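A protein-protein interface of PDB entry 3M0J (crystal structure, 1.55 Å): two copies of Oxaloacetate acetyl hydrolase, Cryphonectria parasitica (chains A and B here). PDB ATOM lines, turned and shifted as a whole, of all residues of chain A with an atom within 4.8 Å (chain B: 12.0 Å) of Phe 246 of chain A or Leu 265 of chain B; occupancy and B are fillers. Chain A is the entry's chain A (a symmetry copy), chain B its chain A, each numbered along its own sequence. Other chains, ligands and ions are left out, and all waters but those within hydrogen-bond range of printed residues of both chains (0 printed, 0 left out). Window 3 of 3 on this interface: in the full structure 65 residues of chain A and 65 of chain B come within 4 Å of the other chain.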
ATOM      1  N   VAL A  28      29.715  -2.773   2.084  1.00  0.00           N
ATOM      2  CA  VAL A  28      29.523  -1.868   0.969  1.00  0.00           C
ATOM      3  C   VAL A  28      30.746  -0.993   0.706  1.00  0.00           C
ATOM      4  O   VAL A  28      31.177  -0.224   1.578  1.00  0.00           O
ATOM      5  CB  VAL A  28      28.277  -1.009   1.185  1.00  0.00           C
ATOM      6  CG1 VAL A  28      28.176   0.075   0.105  1.00  0.00           C
ATOM      7  CG2 VAL A  28      27.032  -1.915   1.226  1.00  0.00           C
ATOM      8  N   CYS A  29      31.304  -1.119  -0.498  1.00  0.00           N
ATOM      9  CA  CYS A  29      32.523  -0.392  -0.861  1.00  0.00           C
ATOM     10  C   CYS A  29      32.310   0.516  -2.043  1.00  0.00           C
ATOM     11  O   CYS A  29      32.235   0.056  -3.171  1.00  0.00           O
ATOM     12  CB  CYS A  29      33.655  -1.362  -1.228  1.00  0.00           C
ATOM     13  SG  CYS A  29      33.907  -2.705  -0.060  1.00  0.00           S
ATOM     14  N   PRO A  30      32.250   1.823  -1.797  1.00  0.00           N
ATOM     15  CA  PRO A  30      32.149   2.757  -2.920  1.00  0.00           C
ATOM     16  C   PRO A  30      33.457   2.736  -3.695  1.00  0.00           C
ATOM     17  O   PRO A  30      34.534   2.667  -3.091  1.00  0.00           O
ATOM     18  CB  PRO A  30      31.964   4.116  -2.224  1.00  0.00           C
ATOM     19  CG  PRO A  30      32.617   3.938  -0.903  1.00  0.00           C
ATOM     20  CD  PRO A  30      32.235   2.517  -0.500  1.00  0.00           C
ATOM     21  N   GLY A  31      33.358   2.794  -5.012  1.00  0.00           N
ATOM     22  CA  GLY A  31      34.533   2.796  -5.849  1.00  0.00           C
ATOM     23  C   GLY A  31      35.148   4.179  -5.925  1.00  0.00           C
ATOM     24  O   GLY A  31      34.508   5.123  -6.393  1.00  0.00           O
ATOM     25  N   PHE A  46      31.953   5.363   5.258  1.00  0.00           N
ATOM     26  CA  PHE A  46      31.932   4.028   4.670  1.00  0.00           C
ATOM     27  C   PHE A  46      32.933   3.141   5.390  1.00  0.00           C
ATOM     28  O   PHE A  46      33.993   3.607   5.801  1.00  0.00           O
ATOM     29  CB  PHE A  46      32.195   4.079   3.169  1.00  0.00           C
ATOM     30  CG  PHE A  46      31.026   4.584   2.390  1.00  0.00           C
ATOM     31  CD1 PHE A  46      30.033   3.716   1.969  1.00  0.00           C
ATOM     32  CD2 PHE A  46      30.893   5.926   2.121  1.00  0.00           C
ATOM     33  CE1 PHE A  46      28.934   4.183   1.255  1.00  0.00           C
ATOM     34  CE2 PHE A  46      29.796   6.403   1.409  1.00  0.00           C
ATOM     35  CZ  PHE A  46      28.814   5.520   0.987  1.00  0.00           C
ATOM     36  N   SER A 222      28.894  -3.835  -8.831  1.00  0.00           N
ATOM     37  CA  SER A 222      27.901  -2.967  -9.431  1.00  0.00           C
ATOM     38  C   SER A 222      28.612  -1.956 -10.312  1.00  0.00           C
ATOM     39  O   SER A 222      29.490  -1.235  -9.848  1.00  0.00           O
ATOM     40  CB  SER A 222      27.101  -2.248  -8.346  1.00  0.00           C
ATOM     41  OG  SER A 222      26.134  -1.386  -8.930  1.00  0.00           O
ATOM     42  N   VAL A 233      21.466  -2.261  -2.810  1.00  0.00           N
ATOM     43  CA  VAL A 233      22.171  -2.806  -1.660  1.00  0.00           C
ATOM     44  C   VAL A 233      21.301  -3.829  -0.950  1.00  0.00           C
ATOM     45  O   VAL A 233      21.764  -4.912  -0.585  1.00  0.00           O
ATOM     46  CB  VAL A 233      22.623  -1.690  -0.685  1.00  0.00           C
ATOM     47  CG1 VAL A 233      22.986  -2.259   0.678  1.00  0.00           C
ATOM     48  CG2 VAL A 233      23.812  -0.927  -1.273  1.00  0.00           C
ATOM     49  N   MET A 244      29.926  -5.812  -1.698  1.00  0.00           N
ATOM     50  CA  MET A 244      29.400  -5.197  -2.906  1.00  0.00           C
ATOM     51  C   MET A 244      30.212  -3.942  -3.188  1.00  0.00           C
ATOM     52  O   MET A 244      30.315  -3.055  -2.336  1.00  0.00           O
ATOM     53  CB  MET A 244      27.919  -4.858  -2.720  1.00  0.00           C
ATOM     54  CG  MET A 244      27.253  -4.261  -3.953  1.00  0.00           C
ATOM     55  SD  MET A 244      25.466  -4.125  -3.693  1.00  0.00           S
ATOM     56  CE  MET A 244      24.920  -3.675  -5.329  1.00  0.00           C
ATOM     57  N   ILE A 245      30.803  -3.879  -4.372  1.00  0.00           N
ATOM     58  CA  ILE A 245      31.608  -2.722  -4.756  1.00  0.00           C
ATOM     59  C   ILE A 245      30.873  -1.943  -5.829  1.00  0.00           C
ATOM     60  O   ILE A 245      30.100  -2.512  -6.612  1.00  0.00           O
ATOM     61  CB  ILE A 245      33.019  -3.111  -5.231  1.00  0.00           C
ATOM     62  CG1 ILE A 245      32.974  -3.851  -6.572  1.00  0.00           C
ATOM     63  CG2 ILE A 245      33.717  -3.977  -4.178  1.00  0.00           C
ATOM     64  CD1 ILE A 245      34.355  -4.260  -7.062  1.00  0.00           C
ATOM     65  N   PHE A 246      31.091  -0.631  -5.841  1.00  0.00           N
ATOM     66  CA  PHE A 246      30.396   0.258  -6.755  1.00  0.00           C
ATOM     67  C   PHE A 246      31.443   0.954  -7.590  1.00  0.00           C
ATOM     68  O   PHE A 246      31.862   2.063  -7.290  1.00  0.00           O
ATOM     69  CB  PHE A 246      29.538   1.247  -5.973  1.00  0.00           C
ATOM     70  CG  PHE A 246      28.373   0.599  -5.298  1.00  0.00           C
ATOM     71  CD1 PHE A 246      27.122   0.624  -5.885  1.00  0.00           C
ATOM     72  CD2 PHE A 246      28.546  -0.092  -4.113  1.00  0.00           C
ATOM     73  CE1 PHE A 246      26.047  -0.011  -5.287  1.00  0.00           C
ATOM     74  CE2 PHE A 246      27.481  -0.712  -3.500  1.00  0.00           C
ATOM     75  CZ  PHE A 246      26.232  -0.676  -4.086  1.00  0.00           C
ATOM     76  N   SER A 247      31.870   0.274  -8.645  1.00  0.00           N
ATOM     77  CA  SER A 247      33.067   0.662  -9.386  1.00  0.00           C
ATOM     78  C   SER A 247      33.091   2.095  -9.901  1.00  0.00           C
ATOM     79  O   SER A 247      34.139   2.738  -9.880  1.00  0.00           O
ATOM     80  CB  SER A 247      33.277  -0.298 -10.551  1.00  0.00           C
ATOM     81  OG  SER A 247      33.692  -1.549 -10.051  1.00  0.00           O
ATOM     82  N   PHE A 248      31.946   2.578 -10.380  1.00  0.00           N
ATOM     83  CA  PHE A 248      31.861   3.897 -11.016  1.00  0.00           C
ATOM     84  C   PHE A 248      31.106   4.915 -10.172  1.00  0.00           C
ATOM     85  O   PHE A 248      30.696   5.967 -10.675  1.00  0.00           O
ATOM     86  CB  PHE A 248      31.231   3.801 -12.413  1.00  0.00           C
ATOM     87  CG  PHE A 248      32.164   3.236 -13.439  1.00  0.00           C
ATOM     88  CD1 PHE A 248      32.771   4.060 -14.374  1.00  0.00           C
ATOM     89  CD2 PHE A 248      32.467   1.884 -13.443  1.00  0.00           C
ATOM     90  CE1 PHE A 248      33.643   3.543 -15.309  1.00  0.00           C
ATOM     91  CE2 PHE A 248      33.350   1.362 -14.368  1.00  0.00           C
ATOM     92  CZ  PHE A 248      33.940   2.194 -15.308  1.00  0.00           C
ATOM     93  N   ALA A 249      30.977   4.627  -8.884  1.00  0.00           N
ATOM     94  CA  ALA A 249      30.175   5.454  -7.967  1.00  0.00           C
ATOM     95  C   ALA A 249      30.671   6.897  -7.825  1.00  0.00           C
ATOM     96  O   ALA A 249      29.903   7.800  -7.485  1.00  0.00           O
ATOM     97  CB  ALA A 249      30.103   4.794  -6.589  1.00  0.00           C
ATOM     98  N   ALA B 256      31.392  18.158  -4.910  1.00  0.00           N
ATOM     99  CA  ALA B 256      29.966  18.303  -4.620  1.00  0.00           C
ATOM    100  C   ALA B 256      29.169  17.088  -5.112  1.00  0.00           C
ATOM    101  O   ALA B 256      28.322  16.546  -4.393  1.00  0.00           O
ATOM    102  CB  ALA B 256      29.421  19.587  -5.258  1.00  0.00           C
ATOM    103  N   ALA B 257      29.459  16.672  -6.342  1.00  0.00           N
ATOM    104  CA  ALA B 257      28.779  15.550  -6.994  1.00  0.00           C
ATOM    105  C   ALA B 257      29.126  14.207  -6.366  1.00  0.00           C
ATOM    106  O   ALA B 257      28.243  13.380  -6.119  1.00  0.00           O
ATOM    107  CB  ALA B 257      29.097  15.540  -8.481  1.00  0.00           C
ATOM    108  N   ILE B 258      30.412  13.979  -6.115  1.00  0.00           N
ATOM    109  CA  ILE B 258      30.840  12.756  -5.447  1.00  0.00           C
ATOM    110  C   ILE B 258      30.176  12.633  -4.079  1.00  0.00           C
ATOM    111  O   ILE B 258      29.648  11.580  -3.733  1.00  0.00           O
ATOM    112  CB  ILE B 258      32.389  12.712  -5.290  1.00  0.00           C
ATOM    113  CG1 ILE B 258      33.043  12.528  -6.665  1.00  0.00           C
ATOM    114  CG2 ILE B 258      32.809  11.576  -4.332  1.00  0.00           C
ATOM    115  CD1 ILE B 258      34.530  12.901  -6.689  1.00  0.00           C
ATOM    116  N   ARG B 259      30.169  13.724  -3.314  1.00  0.00           N
ATOM    117  CA  ARG B 259      29.584  13.678  -1.983  1.00  0.00           C
ATOM    118  C   ARG B 259      28.078  13.394  -2.040  1.00  0.00           C
ATOM    119  O   ARG B 259      27.554  12.573  -1.299  1.00  0.00           O
ATOM    120  CB  ARG B 259      29.847  14.986  -1.233  1.00  0.00           C
ATOM    121  CG  ARG B 259      29.412  14.926   0.226  1.00  0.00           C
ATOM    122  CD  ARG B 259      29.545  16.266   0.922  1.00  0.00           C
ATOM    123  NE  ARG B 259      29.729  16.063   2.354  1.00  0.00           N
ATOM    124  CZ  ARG B 259      28.762  15.673   3.173  1.00  0.00           C
ATOM    125  NH1 ARG B 259      27.543  15.452   2.704  1.00  0.00           N
ATOM    126  NH2 ARG B 259      29.015  15.498   4.458  1.00  0.00           N
ATOM    127  N   GLU B 260      27.368  14.080  -2.926  1.00  0.00           N
ATOM    128  CA  GLU B 260      25.926  13.871  -2.976  1.00  0.00           C
ATOM    129  C   GLU B 260      25.572  12.456  -3.462  1.00  0.00           C
ATOM    130  O   GLU B 260      24.640  11.821  -2.946  1.00  0.00           O
ATOM    131  CB  GLU B 260      25.250  14.982  -3.766  1.00  0.00           C
ATOM    132  CG  GLU B 260      24.835  14.679  -5.161  1.00  0.00           C
ATOM    133  CD  GLU B 260      23.851  15.726  -5.654  1.00  0.00           C
ATOM    134  OE1 GLU B 260      22.735  15.354  -6.071  1.00  0.00           O
ATOM    135  OE2 GLU B 260      24.190  16.927  -5.589  1.00  0.00           O
ATOM    136  N   THR B 261      26.344  11.941  -4.415  1.00  0.00           N
ATOM    137  CA  THR B 261      26.160  10.563  -4.864  1.00  0.00           C
ATOM    138  C   THR B 261      26.423   9.552  -3.751  1.00  0.00           C
ATOM    139  O   THR B 261      25.654   8.608  -3.558  1.00  0.00           O
ATOM    140  CB  THR B 261      27.103  10.237  -6.042  1.00  0.00           C
ATOM    141  OG1 THR B 261      26.815  11.113  -7.141  1.00  0.00           O
ATOM    142  CG2 THR B 261      26.915   8.797  -6.487  1.00  0.00           C
ATOM    143  N   LEU B 262      27.521   9.731  -3.029  1.00  0.00           N
ATOM    144  CA  LEU B 262      27.865   8.773  -1.979  1.00  0.00           C
ATOM    145  C   LEU B 262      26.885   8.835  -0.804  1.00  0.00           C
ATOM    146  O   LEU B 262      26.643   7.830  -0.138  1.00  0.00           O
ATOM    147  CB  LEU B 262      29.314   8.952  -1.508  1.00  0.00           C
ATOM    148  CG  LEU B 262      30.386   8.579  -2.538  1.00  0.00           C
ATOM    149  CD1 LEU B 262      31.768   8.698  -1.910  1.00  0.00           C
ATOM    150  CD2 LEU B 262      30.164   7.166  -3.097  1.00  0.00           C
ATOM    151  N   VAL B 263      26.327  10.011  -0.547  1.00  0.00           N
ATOM    152  CA  VAL B 263      25.273  10.129   0.455  1.00  0.00           C
ATOM    153  C   VAL B 263      24.046   9.332   0.020  1.00  0.00           C
ATOM    154  O   VAL B 263      23.455   8.589   0.807  1.00  0.00           O
ATOM    155  CB  VAL B 263      24.880  11.599   0.703  1.00  0.00           C
ATOM    156  CG1 VAL B 263      23.517  11.665   1.418  1.00  0.00           C
ATOM    157  CG2 VAL B 263      25.961  12.310   1.513  1.00  0.00           C
ATOM    158  N   ARG B 264      23.667   9.483  -1.244  1.00  0.00           N
ATOM    159  CA  ARG B 264      22.570   8.689  -1.803  1.00  0.00           C
ATOM    160  C   ARG B 264      22.857   7.195  -1.678  1.00  0.00           C
ATOM    161  O   ARG B 264      21.983   6.401  -1.328  1.00  0.00           O
ATOM    162  CB  ARG B 264      22.347   9.046  -3.275  1.00  0.00           C
ATOM    163  CG  ARG B 264      21.209   8.270  -3.947  1.00  0.00           C
ATOM    164  CD  ARG B 264      21.016   8.713  -5.398  1.00  0.00           C
ATOM    165  NE  ARG B 264      20.893  10.170  -5.507  1.00  0.00           N
ATOM    166  CZ  ARG B 264      21.753  10.962  -6.150  1.00  0.00           C
ATOM    167  NH1 ARG B 264      22.811  10.460  -6.775  1.00  0.00           N
ATOM    168  NH2 ARG B 264      21.541  12.268  -6.182  1.00  0.00           N
ATOM    169  N   LEU B 265      24.084   6.801  -1.984  1.00  0.00           N
ATOM    170  CA  LEU B 265      24.439   5.388  -1.898  1.00  0.00           C
ATOM    171  C   LEU B 265      24.315   4.912  -0.455  1.00  0.00           C
ATOM    172  O   LEU B 265      23.730   3.872  -0.177  1.00  0.00           O
ATOM    173  CB  LEU B 265      25.852   5.153  -2.422  1.00  0.00           C
ATOM    174  CG  LEU B 265      26.411   3.750  -2.221  1.00  0.00           C
ATOM    175  CD1 LEU B 265      25.438   2.721  -2.770  1.00  0.00           C
ATOM    176  CD2 LEU B 265      27.796   3.609  -2.869  1.00  0.00           C
ATOM    177  N   ARG B 266      24.860   5.695   0.464  1.00  0.00           N
ATOM    178  CA  ARG B 266      24.821   5.349   1.878  1.00  0.00           C
ATOM    179  C   ARG B 266      23.389   5.214   2.395  1.00  0.00           C
ATOM    180  O   ARG B 266      23.041   4.237   3.058  1.00  0.00           O
ATOM    181  CB  ARG B 266      25.572   6.407   2.692  1.00  0.00           C
ATOM    182  CG  ARG B 266      25.752   6.035   4.160  1.00  0.00           C
ATOM    183  CD  ARG B 266      26.314   7.199   4.952  1.00  0.00           C
ATOM    184  NE  ARG B 266      25.361   8.295   4.999  1.00  0.00           N
ATOM    185  CZ  ARG B 266      25.663   9.538   5.366  1.00  0.00           C
ATOM    186  NH1 ARG B 266      26.906   9.852   5.713  1.00  0.00           N
ATOM    187  NH2 ARG B 266      24.716  10.464   5.385  1.00  0.00           N
ATOM    188  N   ASP B 267      22.551   6.183   2.061  1.00  0.00           N
ATOM    189  CA  ASP B 267      21.205   6.250   2.621  1.00  0.00           C
ATOM    190  C   ASP B 267      20.184   5.398   1.874  1.00  0.00           C
ATOM    191  O   ASP B 267      19.218   4.909   2.468  1.00  0.00           O
ATOM    192  CB  ASP B 267      20.724   7.702   2.638  1.00  0.00           C
ATOM    193  CG  ASP B 267      21.458   8.546   3.657  1.00  0.00           C
ATOM    194  OD1 ASP B 267      22.225   7.984   4.468  1.00  0.00           O
ATOM    195  OD2 ASP B 267      21.263   9.773   3.642  1.00  0.00           O
ATOM    196  N   HIS B 268      20.392   5.224   0.572  1.00  0.00           N
ATOM    197  CA  HIS B 268      19.362   4.640  -0.280  1.00  0.00           C
ATOM    198  C   HIS B 268      19.801   3.428  -1.091  1.00  0.00           C
ATOM    199  O   HIS B 268      18.986   2.817  -1.774  1.00  0.00           O
ATOM    200  CB  HIS B 268      18.817   5.703  -1.223  1.00  0.00           C
ATOM    201  CG  HIS B 268      18.085   6.797  -0.520  1.00  0.00           C
ATOM    202  ND1 HIS B 268      16.863   6.597   0.084  1.00  0.00           N
ATOM    203  CD2 HIS B 268      18.402   8.093  -0.311  1.00  0.00           C
ATOM    204  CE1 HIS B 268      16.452   7.729   0.623  1.00  0.00           C
ATOM    205  NE2 HIS B 268      17.365   8.653   0.393  1.00  0.00           N
ATOM    206  N   GLY B 269      21.087   3.101  -1.041  1.00  0.00           N
ATOM    207  CA  GLY B 269      21.578   1.876  -1.652  1.00  0.00           C
ATOM    208  C   GLY B 269      21.659   1.894  -3.162  1.00  0.00           C
ATOM    209  O   GLY B 269      21.759   0.852  -3.800  1.00  0.00           O
ATOM    210  N   VAL B 270      21.629   3.084  -3.744  1.00  0.00           N
ATOM    211  CA  VAL B 270      21.795   3.212  -5.179  1.00  0.00           C
ATOM    212  C   VAL B 270      22.645   4.442  -5.453  1.00  0.00           C
ATOM    213  O   VAL B 270      22.637   5.400  -4.666  1.00  0.00           O
ATOM    214  CB  VAL B 270      20.444   3.364  -5.899  1.00  0.00           C
ATOM    215  CG1 VAL B 270      19.576   2.116  -5.696  1.00  0.00           C
ATOM    216  CG2 VAL B 270      19.728   4.609  -5.404  1.00  0.00           C
ATOM    217  N   VAL B 271      23.368   4.409  -6.568  1.00  0.00           N
ATOM    218  CA  VAL B 271      24.256   5.507  -6.968  1.00  0.00           C
ATOM    219  C   VAL B 271      23.467   6.641  -7.641  1.00  0.00           C
ATOM    220  O   VAL B 271      23.646   7.819  -7.321  1.00  0.00           O
ATOM    221  CB  VAL B 271      25.399   4.994  -7.889  1.00  0.00           C
ATOM    222  CG1 VAL B 271      26.229   6.140  -8.429  1.00  0.00           C
ATOM    223  CG2 VAL B 271      26.296   4.026  -7.131  1.00  0.00           C
ATOM    224  N   GLY B 272      22.584   6.287  -8.570  1.00  0.00           N
ATOM    225  CA  GLY B 272      21.718   7.275  -9.195  1.00  0.00           C
ATOM    226  C   GLY B 272      22.381   8.329 -10.076  1.00  0.00           C
ATOM    227  O   GLY B 272      21.918   9.470 -10.134  1.00  0.00           O
ATOM    228  N   THR B 273      23.444   7.965 -10.779  1.00  0.00           N
ATOM    229  CA  THR B 273      24.087   8.914 -11.688  1.00  0.00           C
ATOM    230  C   THR B 273      23.313   8.945 -13.008  1.00  0.00           C
ATOM    231  O   THR B 273      22.867   7.909 -13.472  1.00  0.00           O
ATOM    232  CB  THR B 273      25.541   8.493 -11.969  1.00  0.00           C
ATOM    233  OG1 THR B 273      26.226   8.323 -10.723  1.00  0.00           O
ATOM    234  CG2 THR B 273      26.256   9.551 -12.789  1.00  0.00           C
ATOM    235  N   ILE B 277      25.803   8.715 -18.491  1.00  0.00           N
ATOM    236  CA  ILE B 277      27.214   8.655 -18.115  1.00  0.00           C
ATOM    237  C   ILE B 277      27.630   7.209 -17.942  1.00  0.00           C
ATOM    238  O   ILE B 277      27.738   6.716 -16.823  1.00  0.00           O
ATOM    239  CB  ILE B 277      27.509   9.419 -16.815  1.00  0.00           C
ATOM    240  CG1 ILE B 277      26.781  10.763 -16.802  1.00  0.00           C
ATOM    241  CG2 ILE B 277      29.025   9.593 -16.626  1.00  0.00           C
ATOM    242  CD1 ILE B 277      27.208  11.694 -17.910  1.00  0.00           C
ATOM    243  N   PRO B 279      30.115   3.715 -18.677  1.00  0.00           N
ATOM    244  CA  PRO B 279      31.543   3.412 -18.762  1.00  0.00           C
ATOM    245  C   PRO B 279      32.103   3.701 -20.141  1.00  0.00           C
ATOM    246  O   PRO B 279      33.169   4.316 -20.230  1.00  0.00           O
ATOM    247  CB  PRO B 279      31.590   1.920 -18.450  1.00  0.00           C
ATOM    248  CG  PRO B 279      30.486   1.772 -17.445  1.00  0.00           C
ATOM    249  CD  PRO B 279      29.379   2.658 -17.967  1.00  0.00           C
ATOM    250  N   LEU B 282      32.644   7.373 -20.707  1.00  0.00           N
ATOM    251  CA  LEU B 282      33.820   7.842 -19.986  1.00  0.00           C
ATOM    252  C   LEU B 282      35.089   7.416 -20.716  1.00  0.00           C
ATOM    253  O   LEU B 282      36.036   8.186 -20.829  1.00  0.00           O
ATOM    254  CB  LEU B 282      33.817   7.335 -18.553  1.00  0.00           C
ATOM    255  CG  LEU B 282      32.659   7.879 -17.718  1.00  0.00           C
ATOM    256  CD1 LEU B 282      32.541   7.073 -16.426  1.00  0.00           C
ATOM    257  CD2 LEU B 282      32.798   9.369 -17.431  1.00  0.00           C
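O of Cys 29 of chain A is in hydrogen-bond range of N of Phe 246 of chain A (3.0 Å). The backbone NH (N) of Leu 265 of chain B lies close to the backbone carbonyl oxygen (O) of Val 270 of chain B, at 3.4 Å. N of Gly 31 of chain A lies within hydrogen-bond range of O of Phe 246 of chain A, 2.8 Å away. OD1 of Asp 267 of chain B lies within salt-bridge range of NE of Arg 266 of chain B (3.2 Å). The backbone carbonyl oxygen (O) of Arg 264 of chain B lies within hydrogen-bond range of the backbone NH (N) of Gly 269 of chain B, at 3.4 Å. NH1 of Arg 264 of chain B sits at hydrogen-bond distance from O of Val 271 of chain B.
Among the printed residues, merely in contact across the chains: Ala 249 of chain A with Thr 261 of chain B, Phe 46 of chain A with Leu 262 of chain B, Pro 30 of chain A with Leu 262 of chain B, Phe 248 of chain A with Leu 282 of chain B, Phe 246 of chain A with Val 271 of chain B, Phe 246 of chain A with Leu 265 of chain B, Phe 46 of chain A with Arg 266 of chain B, Ala 249 of chain A with Val 271 of chain B and Phe 248 of chain A with Pro 279 of chain B.
The backbone carbonyl oxygen (O) of Gly 269 of chain B lies within hydrogen-bond range of the backbone NH (N) of Val 233 of chain A (3.3 Å).
No position is printed for both chains. Of the 10 pairs that touch across the chains among the printed residues, none has its exchanged pair printed and touching as well.
Of the 21 printed residues of chain B, 8 touch a printed residue of chain A. Hydrophobic or aromatic side chains of chain A within 4 Å of the printed part of chain B: Pro 30, Phe 46, Val 233, Phe 246, Phe 248 and Ala 249. Among the printed residues, 10 pairs touch across the chains. Among the printed residues, no Asp or Glu carboxylate lies within 4 Å of a Lys or Arg side-chain nitrogen of the other chain.
Of chain B, only Leu 262 (3.6 Å) comes within 4 Å of Pro 30 of chain A. No residue of chain B comes within 4 Å of Gly 31 of chain A. Of the printed residues of chain B, Phe 46 of chain A touches Leu 262 (3.4 Å) and Arg 266 (3.8 Å). No residue of chain B comes within 4 Å of Ser 222 of chain A. Val 233 of chain A touches just one residue of chain B: Gly 269. No residue of chain B comes within 4 Å of Met 244 of chain A. No residue of chain B comes within 4 Å of Ile 245 of chain A. Ala 249 of chain A touches just these residues of chain B: Thr 261 and Val 271. Of chain A, only Phe 246 (3.7 Å) comes within 4 Å of Leu 265 of chain B. Asp 267 of chain B touches none of the printed residues of chain A. Of the printed residues of chain A, Gly 269 of chain B touches Val 233 (3.3 Å). Printed residues of chain A within 4 Å of Val 271 of chain B: Phe 246 and Ala 249. Gly 272 of chain B touches none of the printed residues of chain A. The nearest printed residue of chain A that does not touch Leu 265 of chain B is Pro 30 of chain A (4.2 Å). The nearest printed residue of chain B that does not touch Phe 46 of chain A is Leu 265 of chain B (4.3 Å).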
